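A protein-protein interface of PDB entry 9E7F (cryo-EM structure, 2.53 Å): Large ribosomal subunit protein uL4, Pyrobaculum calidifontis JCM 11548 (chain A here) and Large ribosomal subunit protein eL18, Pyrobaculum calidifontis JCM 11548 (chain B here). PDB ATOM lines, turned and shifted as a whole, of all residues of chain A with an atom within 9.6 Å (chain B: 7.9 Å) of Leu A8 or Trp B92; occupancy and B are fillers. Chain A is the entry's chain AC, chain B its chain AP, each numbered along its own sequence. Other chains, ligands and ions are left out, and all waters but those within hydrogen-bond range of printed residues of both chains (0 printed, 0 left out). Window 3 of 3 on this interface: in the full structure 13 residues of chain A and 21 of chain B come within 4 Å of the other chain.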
ATOM      1  N   LEU A   8      21.463 -31.453  18.310  1.00  0.00           N
ATOM      2  CA  LEU A   8      21.028 -30.113  18.688  1.00  0.00           C
ATOM      3  C   LEU A   8      19.656 -30.146  19.344  1.00  0.00           C
ATOM      4  O   LEU A   8      19.291 -29.236  20.086  1.00  0.00           O
ATOM      5  CB  LEU A   8      21.002 -29.190  17.467  1.00  0.00           C
ATOM      6  CG  LEU A   8      22.354 -28.660  16.990  1.00  0.00           C
ATOM      7  CD1 LEU A   8      23.182 -28.177  18.168  1.00  0.00           C
ATOM      8  CD2 LEU A   8      23.106 -29.724  16.206  1.00  0.00           C
ATOM      9  N   LEU A   9      18.896 -31.204  19.065  1.00  0.00           N
ATOM     10  CA  LEU A   9      17.566 -31.384  19.623  1.00  0.00           C
ATOM     11  C   LEU A   9      17.551 -32.377  20.781  1.00  0.00           C
ATOM     12  O   LEU A   9      16.496 -32.940  21.090  1.00  0.00           O
ATOM     13  CB  LEU A   9      16.598 -31.832  18.529  1.00  0.00           C
ATOM     14  CG  LEU A   9      16.687 -31.104  17.184  1.00  0.00           C
ATOM     15  CD1 LEU A   9      17.566 -31.862  16.206  1.00  0.00           C
ATOM     16  CD2 LEU A   9      15.301 -30.901  16.600  1.00  0.00           C
ATOM     17  N   LYS A  10      18.700 -32.603  21.424  1.00  0.00           N
ATOM     18  CA  LYS A  10      18.785 -33.623  22.464  1.00  0.00           C
ATOM     19  C   LYS A  10      17.958 -33.247  23.686  1.00  0.00           C
ATOM     20  O   LYS A  10      17.360 -34.117  24.329  1.00  0.00           O
ATOM     21  CB  LYS A  10      20.246 -33.860  22.845  1.00  0.00           C
ATOM     22  CG  LYS A  10      20.955 -32.643  23.399  1.00  0.00           C
ATOM     23  CD  LYS A  10      22.452 -32.727  23.181  1.00  0.00           C
ATOM     24  CE  LYS A  10      23.144 -33.270  24.413  1.00  0.00           C
ATOM     25  NZ  LYS A  10      24.620 -33.167  24.335  1.00  0.00           N
ATOM     26  N   PHE A  11      17.915 -31.962  24.032  1.00  0.00           N
ATOM     27  CA  PHE A  11      17.035 -31.524  25.108  1.00  0.00           C
ATOM     28  C   PHE A  11      15.579 -31.490  24.670  1.00  0.00           C
ATOM     29  O   PHE A  11      14.688 -31.562  25.521  1.00  0.00           O
ATOM     30  CB  PHE A  11      17.449 -30.144  25.610  1.00  0.00           C
ATOM     31  CG  PHE A  11      18.712 -30.144  26.411  1.00  0.00           C
ATOM     32  CD1 PHE A  11      19.941 -30.063  25.788  1.00  0.00           C
ATOM     33  CD2 PHE A  11      18.671 -30.214  27.787  1.00  0.00           C
ATOM     34  CE1 PHE A  11      21.102 -30.062  26.519  1.00  0.00           C
ATOM     35  CE2 PHE A  11      19.833 -30.210  28.528  1.00  0.00           C
ATOM     36  CZ  PHE A  11      21.048 -30.135  27.894  1.00  0.00           C
ATOM     37  N   LYS A  12      15.320 -31.387  23.365  1.00  0.00           N
ATOM     38  CA  LYS A  12      13.944 -31.327  22.885  1.00  0.00           C
ATOM     39  C   LYS A  12      13.262 -32.680  23.016  1.00  0.00           C
ATOM     40  O   LYS A  12      12.322 -32.843  23.802  1.00  0.00           O
ATOM     41  CB  LYS A  12      13.920 -30.861  21.429  1.00  0.00           C
ATOM     42  CG  LYS A  12      12.564 -30.384  20.957  1.00  0.00           C
ATOM     43  CD  LYS A  12      12.705 -29.364  19.856  1.00  0.00           C
ATOM     44  CE  LYS A  12      13.761 -28.346  20.197  1.00  0.00           C
ATOM     45  NZ  LYS A  12      13.182 -27.207  20.946  1.00  0.00           N
ATOM     46  N   LEU A  13      13.737 -33.671  22.268  1.00  0.00           N
ATOM     47  CA  LEU A  13      13.211 -35.028  22.369  1.00  0.00           C
ATOM     48  C   LEU A  13      14.080 -35.755  23.379  1.00  0.00           C
ATOM     49  O   LEU A  13      15.096 -36.359  23.041  1.00  0.00           O
ATOM     50  CB  LEU A  13      13.204 -35.721  21.014  1.00  0.00           C
ATOM     51  CG  LEU A  13      11.970 -36.593  20.769  1.00  0.00           C
ATOM     52  CD1 LEU A  13      10.833 -35.764  20.186  1.00  0.00           C
ATOM     53  CD2 LEU A  13      12.291 -37.780  19.883  1.00  0.00           C
ATOM     54  N   ARG A  26       9.138 -40.425  16.741  1.00  0.00           N
ATOM     55  CA  ARG A  26       8.980 -39.053  16.295  1.00  0.00           C
ATOM     56  C   ARG A  26       8.462 -39.026  14.860  1.00  0.00           C
ATOM     57  O   ARG A  26       8.297 -40.073  14.231  1.00  0.00           O
ATOM     58  CB  ARG A  26      10.312 -38.314  16.422  1.00  0.00           C
ATOM     59  CG  ARG A  26      11.411 -38.863  15.544  1.00  0.00           C
ATOM     60  CD  ARG A  26      12.703 -38.983  16.329  1.00  0.00           C
ATOM     61  NE  ARG A  26      13.167 -37.689  16.818  1.00  0.00           N
ATOM     62  CZ  ARG A  26      14.415 -37.429  17.180  1.00  0.00           C
ATOM     63  NH1 ARG A  26      15.355 -38.357  17.133  1.00  0.00           N
ATOM     64  NH2 ARG A  26      14.726 -36.207  17.601  1.00  0.00           N
ATOM     65  N   ILE A  48      11.713 -28.451  11.226  1.00  0.00           N
ATOM     66  CA  ILE A  48      12.097 -28.517  12.628  1.00  0.00           C
ATOM     67  C   ILE A  48      10.895 -28.411  13.553  1.00  0.00           C
ATOM     68  O   ILE A  48      10.979 -28.792  14.725  1.00  0.00           O
ATOM     69  CB  ILE A  48      13.125 -27.411  12.937  1.00  0.00           C
ATOM     70  CG1 ILE A  48      13.856 -27.708  14.243  1.00  0.00           C
ATOM     71  CG2 ILE A  48      12.445 -26.059  13.002  1.00  0.00           C
ATOM     72  CD1 ILE A  48      14.923 -28.748  14.092  1.00  0.00           C
ATOM     73  N   TYR A  51       9.567 -31.704  15.408  1.00  0.00           N
ATOM     74  CA  TYR A  51      10.335 -32.345  16.466  1.00  0.00           C
ATOM     75  C   TYR A  51      10.037 -31.760  17.835  1.00  0.00           C
ATOM     76  O   TYR A  51      10.604 -32.219  18.829  1.00  0.00           O
ATOM     77  CB  TYR A  51      11.834 -32.244  16.178  1.00  0.00           C
ATOM     78  CG  TYR A  51      12.245 -32.847  14.856  1.00  0.00           C
ATOM     79  CD1 TYR A  51      12.230 -32.092  13.692  1.00  0.00           C
ATOM     80  CD2 TYR A  51      12.640 -34.170  14.769  1.00  0.00           C
ATOM     81  CE1 TYR A  51      12.597 -32.633  12.485  1.00  0.00           C
ATOM     82  CE2 TYR A  51      13.011 -34.724  13.563  1.00  0.00           C
ATOM     83  CZ  TYR A  51      12.987 -33.949  12.423  1.00  0.00           C
ATOM     84  OH  TYR A  51      13.355 -34.487  11.213  1.00  0.00           O
ATOM     85  N   VAL B  51      27.353 -19.616  33.507  1.00  0.00           N
ATOM     86  CA  VAL B  51      28.602 -20.298  33.180  1.00  0.00           C
ATOM     87  C   VAL B  51      29.781 -19.661  33.897  1.00  0.00           C
ATOM     88  O   VAL B  51      30.820 -20.303  34.083  1.00  0.00           O
ATOM     89  CB  VAL B  51      28.814 -20.312  31.660  1.00  0.00           C
ATOM     90  CG1 VAL B  51      27.770 -21.179  31.002  1.00  0.00           C
ATOM     91  CG2 VAL B  51      28.762 -18.906  31.115  1.00  0.00           C
ATOM     92  N   LEU B  70      20.965 -23.888  33.011  1.00  0.00           N
ATOM     93  CA  LEU B  70      22.293 -23.301  32.919  1.00  0.00           C
ATOM     94  C   LEU B  70      22.207 -22.050  32.057  1.00  0.00           C
ATOM     95  O   LEU B  70      21.915 -22.137  30.861  1.00  0.00           O
ATOM     96  CB  LEU B  70      23.296 -24.295  32.336  1.00  0.00           C
ATOM     97  CG  LEU B  70      24.709 -23.749  32.143  1.00  0.00           C
ATOM     98  CD1 LEU B  70      25.316 -23.381  33.478  1.00  0.00           C
ATOM     99  CD2 LEU B  70      25.581 -24.752  31.425  1.00  0.00           C
ATOM    100  N   LEU B  71      22.453 -20.898  32.662  1.00  0.00           N
ATOM    101  CA  LEU B  71      22.362 -19.620  31.977  1.00  0.00           C
ATOM    102  C   LEU B  71      23.742 -19.169  31.517  1.00  0.00           C
ATOM    103  O   LEU B  71      24.763 -19.582  32.066  1.00  0.00           O
ATOM    104  CB  LEU B  71      21.740 -18.563  32.889  1.00  0.00           C
ATOM    105  CG  LEU B  71      20.408 -18.951  33.531  1.00  0.00           C
ATOM    106  CD1 LEU B  71      19.881 -17.834  34.400  1.00  0.00           C
ATOM    107  CD2 LEU B  71      19.397 -19.327  32.470  1.00  0.00           C
ATOM    108  N   GLY B  72      23.766 -18.333  30.486  1.00  0.00           N
ATOM    109  CA  GLY B  72      25.031 -17.844  29.981  1.00  0.00           C
ATOM    110  C   GLY B  72      25.432 -16.506  30.555  1.00  0.00           C
ATOM    111  O   GLY B  72      25.039 -15.460  30.040  1.00  0.00           O
ATOM    112  N   VAL B  82      29.165 -30.644  31.504  1.00  0.00           N
ATOM    113  CA  VAL B  82      28.033 -30.178  32.291  1.00  0.00           C
ATOM    114  C   VAL B  82      26.771 -30.859  31.783  1.00  0.00           C
ATOM    115  O   VAL B  82      26.571 -30.994  30.573  1.00  0.00           O
ATOM    116  CB  VAL B  82      27.902 -28.643  32.255  1.00  0.00           C
ATOM    117  CG1 VAL B  82      29.239 -28.005  32.540  1.00  0.00           C
ATOM    118  CG2 VAL B  82      27.387 -28.158  30.924  1.00  0.00           C
ATOM    119  N   SER B  86      18.173 -27.803  31.339  1.00  0.00           N
ATOM    120  CA  SER B  86      18.088 -27.083  30.080  1.00  0.00           C
ATOM    121  C   SER B  86      19.208 -26.056  30.035  1.00  0.00           C
ATOM    122  O   SER B  86      19.683 -25.582  31.067  1.00  0.00           O
ATOM    123  CB  SER B  86      16.719 -26.422  29.901  1.00  0.00           C
ATOM    124  OG  SER B  86      16.516 -25.381  30.834  1.00  0.00           O
ATOM    125  N   VAL B  87      19.628 -25.724  28.817  1.00  0.00           N
ATOM    126  CA  VAL B  87      20.764 -24.845  28.576  1.00  0.00           C
ATOM    127  C   VAL B  87      20.350 -23.778  27.575  1.00  0.00           C
ATOM    128  O   VAL B  87      19.764 -24.092  26.536  1.00  0.00           O
ATOM    129  CB  VAL B  87      21.981 -25.629  28.052  1.00  0.00           C
ATOM    130  CG1 VAL B  87      23.187 -24.732  27.939  1.00  0.00           C
ATOM    131  CG2 VAL B  87      22.278 -26.805  28.952  1.00  0.00           C
ATOM    132  N   THR B  88      20.657 -22.522  27.883  1.00  0.00           N
ATOM    133  CA  THR B  88      20.426 -21.451  26.932  1.00  0.00           C
ATOM    134  C   THR B  88      21.441 -21.542  25.797  1.00  0.00           C
ATOM    135  O   THR B  88      22.479 -22.189  25.935  1.00  0.00           O
ATOM    136  CB  THR B  88      20.522 -20.092  27.618  1.00  0.00           C
ATOM    137  OG1 THR B  88      21.866 -19.868  28.060  1.00  0.00           O
ATOM    138  CG2 THR B  88      19.598 -20.038  28.816  1.00  0.00           C
ATOM    139  N   PRO B  89      21.142 -20.933  24.647  1.00  0.00           N
ATOM    140  CA  PRO B  89      22.095 -20.978  23.524  1.00  0.00           C
ATOM    141  C   PRO B  89      23.432 -20.327  23.827  1.00  0.00           C
ATOM    142  O   PRO B  89      24.463 -20.761  23.304  1.00  0.00           O
ATOM    143  CB  PRO B  89      21.344 -20.247  22.405  1.00  0.00           C
ATOM    144  CG  PRO B  89      19.914 -20.348  22.775  1.00  0.00           C
ATOM    145  CD  PRO B  89      19.869 -20.305  24.266  1.00  0.00           C
ATOM    146  N   LYS B  90      23.445 -19.292  24.665  1.00  0.00           N
ATOM    147  CA  LYS B  90      24.704 -18.660  25.040  1.00  0.00           C
ATOM    148  C   LYS B  90      25.512 -19.546  25.981  1.00  0.00           C
ATOM    149  O   LYS B  90      26.743 -19.579  25.901  1.00  0.00           O
ATOM    150  CB  LYS B  90      24.435 -17.301  25.682  1.00  0.00           C
ATOM    151  CG  LYS B  90      25.668 -16.611  26.223  1.00  0.00           C
ATOM    152  CD  LYS B  90      25.321 -15.254  26.791  1.00  0.00           C
ATOM    153  CE  LYS B  90      26.424 -14.256  26.527  1.00  0.00           C
ATOM    154  NZ  LYS B  90      25.981 -13.145  25.642  1.00  0.00           N
ATOM    155  N   ALA B  91      24.841 -20.260  26.887  1.00  0.00           N
ATOM    156  CA  ALA B  91      25.548 -21.157  27.794  1.00  0.00           C
ATOM    157  C   ALA B  91      26.162 -22.336  27.050  1.00  0.00           C
ATOM    158  O   ALA B  91      27.285 -22.752  27.353  1.00  0.00           O
ATOM    159  CB  ALA B  91      24.602 -21.652  28.882  1.00  0.00           C
ATOM    160  N   TRP B  92      25.429 -22.899  26.087  1.00  0.00           N
ATOM    161  CA  TRP B  92      25.949 -24.007  25.291  1.00  0.00           C
ATOM    162  C   TRP B  92      27.158 -23.564  24.477  1.00  0.00           C
ATOM    163  O   TRP B  92      28.138 -24.305  24.357  1.00  0.00           O
ATOM    164  CB  TRP B  92      24.835 -24.548  24.384  1.00  0.00           C
ATOM    165  CG  TRP B  92      25.045 -25.904  23.695  1.00  0.00           C
ATOM    166  CD1 TRP B  92      26.226 -26.514  23.379  1.00  0.00           C
ATOM    167  CD2 TRP B  92      24.014 -26.775  23.209  1.00  0.00           C
ATOM    168  NE1 TRP B  92      25.997 -27.707  22.747  1.00  0.00           N
ATOM    169  CE2 TRP B  92      24.647 -27.892  22.628  1.00  0.00           C
ATOM    170  CE3 TRP B  92      22.616 -26.722  23.216  1.00  0.00           C
ATOM    171  CZ2 TRP B  92      23.932 -28.946  22.063  1.00  0.00           C
ATOM    172  CZ3 TRP B  92      21.908 -27.768  22.650  1.00  0.00           C
ATOM    173  CH2 TRP B  92      22.567 -28.865  22.084  1.00  0.00           C
ATOM    174  N   LYS B  93      27.100 -22.367  23.893  1.00  0.00           N
ATOM    175  CA  LYS B  93      28.225 -21.889  23.099  1.00  0.00           C
ATOM    176  C   LYS B  93      29.446 -21.626  23.971  1.00  0.00           C
ATOM    177  O   LYS B  93      30.569 -21.974  23.597  1.00  0.00           O
ATOM    178  CB  LYS B  93      27.821 -20.630  22.332  1.00  0.00           C
ATOM    179  CG  LYS B  93      28.936 -20.009  21.526  1.00  0.00           C
ATOM    180  CD  LYS B  93      28.889 -18.496  21.579  1.00  0.00           C
ATOM    181  CE  LYS B  93      27.477 -17.975  21.405  1.00  0.00           C
ATOM    182  NZ  LYS B  93      27.426 -16.486  21.354  1.00  0.00           N
ATOM    183  N   LYS B  94      29.247 -21.032  25.146  1.00  0.00           N
ATOM    184  CA  LYS B  94      30.378 -20.734  26.014  1.00  0.00           C
ATOM    185  C   LYS B  94      30.996 -21.998  26.594  1.00  0.00           C
ATOM    186  O   LYS B  94      32.208 -22.040  26.823  1.00  0.00           O
ATOM    187  CB  LYS B  94      29.953 -19.785  27.130  1.00  0.00           C
ATOM    188  CG  LYS B  94      29.831 -18.347  26.677  1.00  0.00           C
ATOM    189  CD  LYS B  94      29.420 -17.437  27.805  1.00  0.00           C
ATOM    190  CE  LYS B  94      29.249 -16.017  27.315  1.00  0.00           C
ATOM    191  NZ  LYS B  94      28.834 -15.115  28.416  1.00  0.00           N
ATOM    192  N   VAL B  95      30.185 -23.026  26.855  1.00  0.00           N
ATOM    193  CA  VAL B  95      30.723 -24.283  27.364  1.00  0.00           C
ATOM    194  C   VAL B  95      31.504 -25.010  26.282  1.00  0.00           C
ATOM    195  O   VAL B  95      32.568 -25.581  26.543  1.00  0.00           O
ATOM    196  CB  VAL B  95      29.594 -25.162  27.924  1.00  0.00           C
ATOM    197  CG1 VAL B  95      29.974 -26.622  27.815  1.00  0.00           C
ATOM    198  CG2 VAL B  95      29.305 -24.791  29.362  1.00  0.00           C
ATOM    199  N   VAL B  96      30.982 -25.021  25.058  1.00  0.00           N
ATOM    200  CA  VAL B  96      31.628 -25.756  23.975  1.00  0.00           C
ATOM    201  C   VAL B  96      32.942 -25.095  23.587  1.00  0.00           C
ATOM    202  O   VAL B  96      33.968 -25.763  23.428  1.00  0.00           O
ATOM    203  CB  VAL B  96      30.678 -25.872  22.771  1.00  0.00           C
ATOM    204  CG1 VAL B  96      31.451 -26.266  21.536  1.00  0.00           C
ATOM    205  CG2 VAL B  96      29.590 -26.883  23.057  1.00  0.00           C
ATOM    206  N   GLU B  97      32.935 -23.770  23.438  1.00  0.00           N
ATOM    207  CA  GLU B  97      34.130 -23.063  23.001  1.00  0.00           C
ATOM    208  C   GLU B  97      35.207 -23.009  24.073  1.00  0.00           C
ATOM    209  O   GLU B  97      36.358 -22.707  23.750  1.00  0.00           O
ATOM    210  CB  GLU B  97      33.767 -21.651  22.543  1.00  0.00           C
ATOM    211  CG  GLU B  97      33.505 -21.570  21.046  1.00  0.00           C
ATOM    212  CD  GLU B  97      32.317 -20.698  20.697  1.00  0.00           C
ATOM    213  OE1 GLU B  97      32.216 -19.578  21.238  1.00  0.00           O
ATOM    214  OE2 GLU B  97      31.477 -21.138  19.889  1.00  0.00           O
ATOM    215  N   ALA B  98      34.866 -23.292  25.326  1.00  0.00           N
ATOM    216  CA  ALA B  98      35.846 -23.434  26.389  1.00  0.00           C
ATOM    217  C   ALA B  98      36.450 -24.828  26.441  1.00  0.00           C
ATOM    218  O   ALA B  98      37.317 -25.080  27.281  1.00  0.00           O
ATOM    219  CB  ALA B  98      35.214 -23.097  27.739  1.00  0.00           C
ATOM    220  N   GLY B 100      34.528 -27.635  26.895  1.00  0.00           N
ATOM    221  CA  GLY B 100      33.618 -28.523  27.580  1.00  0.00           C
ATOM    222  C   GLY B 100      32.620 -29.162  26.635  1.00  0.00           C
ATOM    223  O   GLY B 100      32.708 -29.059  25.414  1.00  0.00           O
ATOM    224  N   GLU B 101      31.653 -29.850  27.228  1.00  0.00           N
ATOM    225  CA  GLU B 101      30.619 -30.529  26.468  1.00  0.00           C
ATOM    226  C   GLU B 101      29.351 -30.586  27.302  1.00  0.00           C
ATOM    227  O   GLU B 101      29.408 -30.815  28.511  1.00  0.00           O
ATOM    228  CB  GLU B 101      31.084 -31.927  26.055  1.00  0.00           C
ATOM    229  CG  GLU B 101      31.061 -32.953  27.156  1.00  0.00           C
ATOM    230  CD  GLU B 101      30.641 -34.313  26.658  1.00  0.00           C
ATOM    231  OE1 GLU B 101      29.841 -34.370  25.704  1.00  0.00           O
ATOM    232  OE2 GLU B 101      31.104 -35.326  27.225  1.00  0.00           O
ATOM    233  N   VAL B 102      28.213 -30.361  26.657  1.00  0.00           N
ATOM    234  CA  VAL B 102      26.935 -30.231  27.342  1.00  0.00           C
ATOM    235  C   VAL B 102      26.138 -31.514  27.164  1.00  0.00           C
ATOM    236  O   VAL B 102      25.957 -31.994  26.037  1.00  0.00           O
ATOM    237  CB  VAL B 102      26.147 -29.016  26.828  1.00  0.00           C
ATOM    238  CG1 VAL B 102      24.827 -28.905  27.557  1.00  0.00           C
ATOM    239  CG2 VAL B 102      26.953 -27.759  27.023  1.00  0.00           C
ATOM    240  N   LEU B 103      25.650 -32.056  28.275  1.00  0.00           N
ATOM    241  CA  LEU B 103      24.932 -33.318  28.313  1.00  0.00           C
ATOM    242  C   LEU B 103      23.537 -33.109  28.873  1.00  0.00           C
ATOM    243  O   LEU B 103      23.309 -32.214  29.688  1.00  0.00           O
ATOM    244  CB  LEU B 103      25.655 -34.339  29.186  1.00  0.00           C
ATOM    245  CG  LEU B 103      26.574 -35.334  28.504  1.00  0.00           C
ATOM    246  CD1 LEU B 103      27.493 -34.586  27.595  1.00  0.00           C
ATOM    247  CD2 LEU B 103      27.356 -36.096  29.547  1.00  0.00           C
ATOM    248  N   THR B 104      22.603 -33.941  28.433  1.00  0.00           N
ATOM    249  CA  THR B 104      21.343 -34.053  29.145  1.00  0.00           C
ATOM    250  C   THR B 104      21.558 -34.879  30.407  1.00  0.00           C
ATOM    251  O   THR B 104      22.495 -35.674  30.500  1.00  0.00           O
ATOM    252  CB  THR B 104      20.262 -34.690  28.272  1.00  0.00           C
ATOM    253  OG1 THR B 104      20.551 -36.078  28.078  1.00  0.00           O
ATOM    254  CG2 THR B 104      20.184 -34.002  26.923  1.00  0.00           C
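Printed residues of chain A that touch a printed residue of chain B: Leu A8, Lys A10 and Phe A11. Hydrophobic or aromatic side chains of chain A within 4 Å of the printed part of chain B: Phe A11. Along chain A the printed residues that touch a printed residue of chain B span positions 8 to 11. Hydrophobic or aromatic side chains of chain B that line the printed part of chain A: Val B87, Trp B92 and Val B102.
Leu A8 touches one residue of chain B. Printed residues of chain A within 4 Å of Trp B92: Leu A8 (3.9 Å). No residue of chain A comes within 4 Å of Val B95. Of the printed residues of chain A, Val B102 touches Lys A10 (2.5 Å) and Phe A11 (3.99 Å). Printed residues of chain A within 4 Å of Val B87: Phe A11. Of the printed residues of chain B, Lys A10 touches Val B102 (2.5 Å), Leu B103 (3.99 Å) and Thr B104 (3.8 Å). Of the printed residues of chain B, Phe A11 touches Ser B86, Val B87, Val B102 and Leu B103. Lys A12 touches none of the printed residues of chain B. Lys B94 touches none of the printed residues of chain A. The nearest printed residue of chain B that does not touch Leu A8 is Val B96 (8.2 Å). The nearest printed residue of chain A that does not touch Val B102 is Leu A8 (9.0 Å).
O of Ser B86 sits at hydrogen-bond distance from N of Leu B70, at 2.9 Å. The backbone carbonyl oxygen of Val B82 lies within hydrogen-bond range of the backbone NH of Leu B103 (2.7 Å).
The backbone carbonyl oxygen (O) of Val B102 is in hydrogen-bond range of the side-chain amino group (NZ) of Lys A10.
Among the printed residues, pairs that only touch across the chains: Phe A11 with Leu B103 (3.6 Å), Phe A11 with Val B87 (3.7 Å), Lys A10 with Thr B104 (3.8 Å), Leu A8 with Trp B92 (3.9 Å), Phe A11 with Ser B86 (3.9 Å), Phe A11 with Val B102 (3.99 Å) and Lys A10 with Leu B103 (3.99 Å).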
